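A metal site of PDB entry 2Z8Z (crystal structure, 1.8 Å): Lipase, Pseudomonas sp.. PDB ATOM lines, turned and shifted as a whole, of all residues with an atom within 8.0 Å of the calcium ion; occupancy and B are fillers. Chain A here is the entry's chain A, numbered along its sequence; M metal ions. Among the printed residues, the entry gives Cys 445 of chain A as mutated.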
ATOM      1  N   THR A 369      -6.321 -16.813  19.206  1.00  0.00           N
ATOM      2  CA  THR A 369      -7.551 -17.532  18.920  1.00  0.00           C
ATOM      3  C   THR A 369      -7.275 -19.030  19.121  1.00  0.00           C
ATOM      4  O   THR A 369      -6.277 -19.548  18.621  1.00  0.00           O
ATOM      5  CB  THR A 369      -8.065 -17.269  17.525  1.00  0.00           C
ATOM      6  OG1 THR A 369      -8.159 -15.844  17.294  1.00  0.00           O
ATOM      7  CG2 THR A 369      -9.428 -17.943  17.318  1.00  0.00           C
ATOM      8  N   GLN A 381      -9.528 -23.865  10.029  1.00  0.00           N
ATOM      9  CA  GLN A 381      -8.817 -22.748   9.412  1.00  0.00           C
ATOM     10  C   GLN A 381      -8.469 -21.629  10.453  1.00  0.00           C
ATOM     11  O   GLN A 381      -9.366 -20.981  10.994  1.00  0.00           O
ATOM     12  CB  GLN A 381      -9.695 -22.170   8.302  1.00  0.00           C
ATOM     13  CG  GLN A 381      -9.359 -20.831   7.773  1.00  0.00           C
ATOM     14  CD  GLN A 381      -8.295 -20.843   6.709  1.00  0.00           C
ATOM     15  OE1 GLN A 381      -8.498 -21.332   5.596  1.00  0.00           O
ATOM     16  NE2 GLN A 381      -7.163 -20.204   7.009  1.00  0.00           N
ATOM     17  N   GLY A 382      -7.185 -21.401  10.706  1.00  0.00           N
ATOM     18  CA  GLY A 382      -6.797 -20.302  11.548  1.00  0.00           C
ATOM     19  C   GLY A 382      -6.605 -19.041  10.760  1.00  0.00           C
ATOM     20  O   GLY A 382      -6.416 -19.056   9.537  1.00  0.00           O
ATOM     21  N   GLY A 383      -6.617 -17.920  11.473  1.00  0.00           N
ATOM     22  CA  GLY A 383      -6.621 -16.617  10.847  1.00  0.00           C
ATOM     23  C   GLY A 383      -5.193 -16.175  10.635  1.00  0.00           C
ATOM     24  O   GLY A 383      -4.288 -16.975  10.756  1.00  0.00           O
ATOM     25  N   SER A 384      -5.044 -14.905  10.311  1.00  0.00           N
ATOM     26  CA  SER A 384      -3.744 -14.311   9.990  1.00  0.00           C
ATOM     27  C   SER A 384      -3.025 -13.803  11.211  1.00  0.00           C
ATOM     28  O   SER A 384      -1.853 -13.445  11.126  1.00  0.00           O
ATOM     29  CB  SER A 384      -3.883 -13.188   8.956  1.00  0.00           C
ATOM     30  OG  SER A 384      -4.651 -12.157   9.479  1.00  0.00           O
ATOM     31  N   GLY A 385      -3.701 -13.825  12.357  1.00  0.00           N
ATOM     32  CA  GLY A 385      -3.095 -13.622  13.647  1.00  0.00           C
ATOM     33  C   GLY A 385      -2.560 -14.952  14.216  1.00  0.00           C
ATOM     34  O   GLY A 385      -2.378 -15.941  13.516  1.00  0.00           O
ATOM     35  N   ASN A 386      -2.421 -14.971  15.529  1.00  0.00           N
ATOM     36  CA  ASN A 386      -1.867 -16.090  16.260  1.00  0.00           C
ATOM     37  C   ASN A 386      -2.979 -17.057  16.729  1.00  0.00           C
ATOM     38  O   ASN A 386      -3.971 -16.637  17.294  1.00  0.00           O
ATOM     39  CB  ASN A 386      -1.065 -15.532  17.449  1.00  0.00           C
ATOM     40  CG  ASN A 386      -0.065 -14.461  17.036  1.00  0.00           C
ATOM     41  OD1 ASN A 386       0.543 -14.513  15.938  1.00  0.00           O
ATOM     42  ND2 ASN A 386       0.019 -13.427  17.869  1.00  0.00           N
ATOM     43  N   ASP A 387      -2.778 -18.344  16.436  1.00  0.00           N
ATOM     44  CA  ASP A 387      -3.845 -19.376  16.590  1.00  0.00           C
ATOM     45  C   ASP A 387      -3.277 -20.606  17.259  1.00  0.00           C
ATOM     46  O   ASP A 387      -2.118 -20.994  17.036  1.00  0.00           O
ATOM     47  CB  ASP A 387      -4.442 -19.823  15.223  1.00  0.00           C
ATOM     48  CG  ASP A 387      -5.117 -18.703  14.533  1.00  0.00           C
ATOM     49  OD1 ASP A 387      -6.332 -18.598  14.655  1.00  0.00           O
ATOM     50  OD2 ASP A 387      -4.439 -17.893  13.897  1.00  0.00           O
ATOM     51  N   TYR A 388      -4.147 -21.222  18.052  1.00  0.00           N
ATOM     52  CA  TYR A 388      -3.898 -22.517  18.664  1.00  0.00           C
ATOM     53  C   TYR A 388      -4.980 -23.465  18.162  1.00  0.00           C
ATOM     54  O   TYR A 388      -6.130 -23.367  18.543  1.00  0.00           O
ATOM     55  CB  TYR A 388      -3.908 -22.419  20.169  1.00  0.00           C
ATOM     56  CG  TYR A 388      -2.850 -21.479  20.683  1.00  0.00           C
ATOM     57  CD1 TYR A 388      -1.578 -21.945  21.035  1.00  0.00           C
ATOM     58  CD2 TYR A 388      -3.110 -20.108  20.795  1.00  0.00           C
ATOM     59  CE1 TYR A 388      -0.617 -21.060  21.500  1.00  0.00           C
ATOM     60  CE2 TYR A 388      -2.131 -19.215  21.268  1.00  0.00           C
ATOM     61  CZ  TYR A 388      -0.880 -19.705  21.579  1.00  0.00           C
ATOM     62  OH  TYR A 388       0.104 -18.853  22.053  1.00  0.00           O
ATOM     63  N   LEU A 389      -4.609 -24.401  17.299  1.00  0.00           N
ATOM     64  CA  LEU A 389      -5.554 -25.236  16.584  1.00  0.00           C
ATOM     65  C   LEU A 389      -5.406 -26.650  17.081  1.00  0.00           C
ATOM     66  O   LEU A 389      -4.290 -27.176  17.094  1.00  0.00           O
ATOM     67  CB  LEU A 389      -5.214 -25.239  15.077  1.00  0.00           C
ATOM     68  CG  LEU A 389      -5.109 -23.866  14.418  1.00  0.00           C
ATOM     69  CD1 LEU A 389      -4.870 -23.908  12.915  1.00  0.00           C
ATOM     70  CD2 LEU A 389      -6.322 -22.936  14.740  1.00  0.00           C
ATOM     71  N   ARG A 399      -5.559 -25.377   7.901  1.00  0.00           N
ATOM     72  CA  ARG A 399      -5.114 -24.276   7.119  1.00  0.00           C
ATOM     73  C   ARG A 399      -4.827 -23.206   8.136  1.00  0.00           C
ATOM     74  O   ARG A 399      -5.421 -23.171   9.217  1.00  0.00           O
ATOM     75  CB  ARG A 399      -6.191 -23.793   6.125  1.00  0.00           C
ATOM     76  CG  ARG A 399      -6.304 -24.723   4.920  1.00  0.00           C
ATOM     77  CD  ARG A 399      -7.421 -24.337   4.048  1.00  0.00           C
ATOM     78  NE  ARG A 399      -7.321 -24.999   2.768  1.00  0.00           N
ATOM     79  CZ  ARG A 399      -8.215 -24.874   1.793  1.00  0.00           C
ATOM     80  NH1 ARG A 399      -9.265 -24.108   1.937  1.00  0.00           N
ATOM     81  NH2 ARG A 399      -8.017 -25.535   0.646  1.00  0.00           N
ATOM     82  N   ASP A 400      -3.988 -22.266   7.777  1.00  0.00           N
ATOM     83  CA  ASP A 400      -3.812 -21.124   8.668  1.00  0.00           C
ATOM     84  C   ASP A 400      -3.256 -19.959   7.887  1.00  0.00           C
ATOM     85  O   ASP A 400      -2.384 -20.170   7.035  1.00  0.00           O
ATOM     86  CB  ASP A 400      -2.894 -21.471   9.862  1.00  0.00           C
ATOM     87  CG  ASP A 400      -2.700 -20.274  10.793  1.00  0.00           C
ATOM     88  OD1 ASP A 400      -3.516 -20.043  11.720  1.00  0.00           O
ATOM     89  OD2 ASP A 400      -1.784 -19.519  10.534  1.00  0.00           O
ATOM     90  N   GLY A 401      -3.701 -18.780   8.246  1.00  0.00           N
ATOM     91  CA  GLY A 401      -3.479 -17.526   7.479  1.00  0.00           C
ATOM     92  C   GLY A 401      -2.190 -16.768   7.809  1.00  0.00           C
ATOM     93  O   GLY A 401      -1.900 -15.772   7.191  1.00  0.00           O
ATOM     94  N   GLY A 402      -1.420 -17.243   8.784  1.00  0.00           N
ATOM     95  CA  GLY A 402      -0.152 -16.623   9.114  1.00  0.00           C
ATOM     96  C   GLY A 402       0.062 -16.442  10.577  1.00  0.00           C
ATOM     97  O   GLY A 402      -0.673 -16.961  11.390  1.00  0.00           O
ATOM     98  N   GLY A 403       1.051 -15.657  10.933  1.00  0.00           N
ATOM     99  CA  GLY A 403       1.309 -15.369  12.340  1.00  0.00           C
ATOM    100  C   GLY A 403       2.093 -16.482  13.008  1.00  0.00           C
ATOM    101  O   GLY A 403       2.790 -17.256  12.346  1.00  0.00           O
ATOM    102  N   TYR A 404       2.001 -16.536  14.329  1.00  0.00           N
ATOM    103  CA  TYR A 404       2.681 -17.573  15.151  1.00  0.00           C
ATOM    104  C   TYR A 404       1.633 -18.523  15.731  1.00  0.00           C
ATOM    105  O   TYR A 404       0.635 -18.091  16.241  1.00  0.00           O
ATOM    106  CB  TYR A 404       3.457 -16.875  16.249  1.00  0.00           C
ATOM    107  CG  TYR A 404       4.506 -15.957  15.669  1.00  0.00           C
ATOM    108  CD1 TYR A 404       5.784 -16.387  15.425  1.00  0.00           C
ATOM    109  CD2 TYR A 404       4.173 -14.663  15.218  1.00  0.00           C
ATOM    110  CE1 TYR A 404       6.738 -15.530  14.830  1.00  0.00           C
ATOM    111  CE2 TYR A 404       5.135 -13.833  14.635  1.00  0.00           C
ATOM    112  CZ  TYR A 404       6.383 -14.278  14.454  1.00  0.00           C
ATOM    113  OH  TYR A 404       7.369 -13.514  13.880  1.00  0.00           O
ATOM    114  N   ASN A 405       1.818 -19.839  15.603  1.00  0.00           N
ATOM    115  CA  ASN A 405       0.695 -20.732  15.835  1.00  0.00           C
ATOM    116  C   ASN A 405       1.192 -22.033  16.411  1.00  0.00           C
ATOM    117  O   ASN A 405       2.324 -22.407  16.210  1.00  0.00           O
ATOM    118  CB  ASN A 405      -0.001 -21.039  14.508  1.00  0.00           C
ATOM    119  CG  ASN A 405      -0.344 -19.805  13.699  1.00  0.00           C
ATOM    120  OD1 ASN A 405      -1.381 -19.165  13.921  1.00  0.00           O
ATOM    121  ND2 ASN A 405       0.502 -19.483  12.699  1.00  0.00           N
ATOM    122  N   VAL A 406       0.303 -22.733  17.109  1.00  0.00           N
ATOM    123  CA  VAL A 406       0.562 -24.096  17.499  1.00  0.00           C
ATOM    124  C   VAL A 406      -0.568 -24.962  16.938  1.00  0.00           C
ATOM    125  O   VAL A 406      -1.732 -24.631  17.063  1.00  0.00           O
ATOM    126  CB  VAL A 406       0.681 -24.293  19.004  1.00  0.00           C
ATOM    127  CG1 VAL A 406       0.989 -25.741  19.336  1.00  0.00           C
ATOM    128  CG2 VAL A 406       1.722 -23.401  19.618  1.00  0.00           C
ATOM    129  N   ILE A 407      -0.178 -26.060  16.272  1.00  0.00           N
ATOM    130  CA  ILE A 407      -1.151 -26.941  15.620  1.00  0.00           C
ATOM    131  C   ILE A 407      -0.925 -28.321  16.147  1.00  0.00           C
ATOM    132  O   ILE A 407       0.156 -28.911  15.932  1.00  0.00           O
ATOM    133  CB  ILE A 407      -1.027 -26.965  14.095  1.00  0.00           C
ATOM    134  CG1 ILE A 407      -1.113 -25.528  13.590  1.00  0.00           C
ATOM    135  CG2 ILE A 407      -2.087 -27.833  13.475  1.00  0.00           C
ATOM    136  CD1 ILE A 407      -0.924 -25.295  12.116  1.00  0.00           C
ATOM    137  N   ASP A 439       6.933 -19.415   7.619  1.00  0.00           N
ATOM    138  CA  ASP A 439       6.507 -18.772   6.403  1.00  0.00           C
ATOM    139  C   ASP A 439       7.479 -17.706   5.947  1.00  0.00           C
ATOM    140  O   ASP A 439       8.502 -17.440   6.626  1.00  0.00           O
ATOM    141  CB  ASP A 439       5.037 -18.298   6.469  1.00  0.00           C
ATOM    142  CG  ASP A 439       4.782 -17.081   7.403  1.00  0.00           C
ATOM    143  OD1 ASP A 439       5.675 -16.205   7.575  1.00  0.00           O
ATOM    144  OD2 ASP A 439       3.606 -16.978   7.903  1.00  0.00           O
ATOM    145  N   ILE A 444       5.985 -18.422  12.616  1.00  0.00           N
ATOM    146  CA  ILE A 444       6.327 -19.792  12.951  1.00  0.00           C
ATOM    147  C   ILE A 444       5.136 -20.558  13.545  1.00  0.00           C
ATOM    148  O   ILE A 444       4.446 -20.014  14.419  1.00  0.00           O
ATOM    149  CB  ILE A 444       7.463 -19.846  13.997  1.00  0.00           C
ATOM    150  CG1 ILE A 444       8.752 -19.187  13.449  1.00  0.00           C
ATOM    151  CG2 ILE A 444       7.776 -21.338  14.394  1.00  0.00           C
ATOM    152  CD1 ILE A 444       9.814 -19.034  14.483  1.00  0.00           C
ATOM    153  N   CYS A 445       4.897 -21.784  13.034  1.00  0.00           N
ATOM    154  CA  CYS A 445       3.936 -22.776  13.528  1.00  0.00           C
ATOM    155  C   CYS A 445       4.761 -23.839  14.212  1.00  0.00           C
ATOM    156  O   CYS A 445       5.759 -24.344  13.637  1.00  0.00           O
ATOM    157  CB  CYS A 445       3.138 -23.416  12.359  1.00  0.00           C
ATOM    158  SG  CYS A 445       2.177 -22.096  11.736  1.00  0.00           S
HETATM  159 CA    CA M   1      -2.670 -17.868  12.404  1.00  0.00          CA
HETATM  160 PT    PT M   2       1.451 -22.872   9.694  1.00  0.00          PT
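The calcium ion is bound by O of Gly 385 (2.2 Å), OD2 of Asp 387 (2.3 Å), OD1 of Asn 405 (2.4 Å), O of Gly 402 (2.4 Å), OD1 of Asp 400 (2.4 Å), O of Gly 383 (2.5 Å) and OD2 of Asp 400 (2.6 Å).
Along chain A the residues within 4 Å of the calcium ion span positions 383 to 405.
The backbone NH (N) of Asp 387 is in hydrogen-bond range of the backbone carbonyl oxygen (O) of Tyr 404 (3.4 Å).
N of Val 406 is in hydrogen-bond range of O of Asp 387, at 3.0 Å.
The side-chain amide nitrogen of Asn 405 sits at hydrogen-bond distance from the backbone carbonyl oxygen of Gly 403.
The side-chain sulfur (SG) of Cys 445 lies close to the side-chain amide nitrogen (ND2) of Asn 405 (3.2 Å).
The backbone carbonyl oxygen (O) of Ile 444 lies within hydrogen-bond range of the backbone NH (N) of Asn 405, at 2.9 Å.
O of Gly 383 lies close to N of Gly 401.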
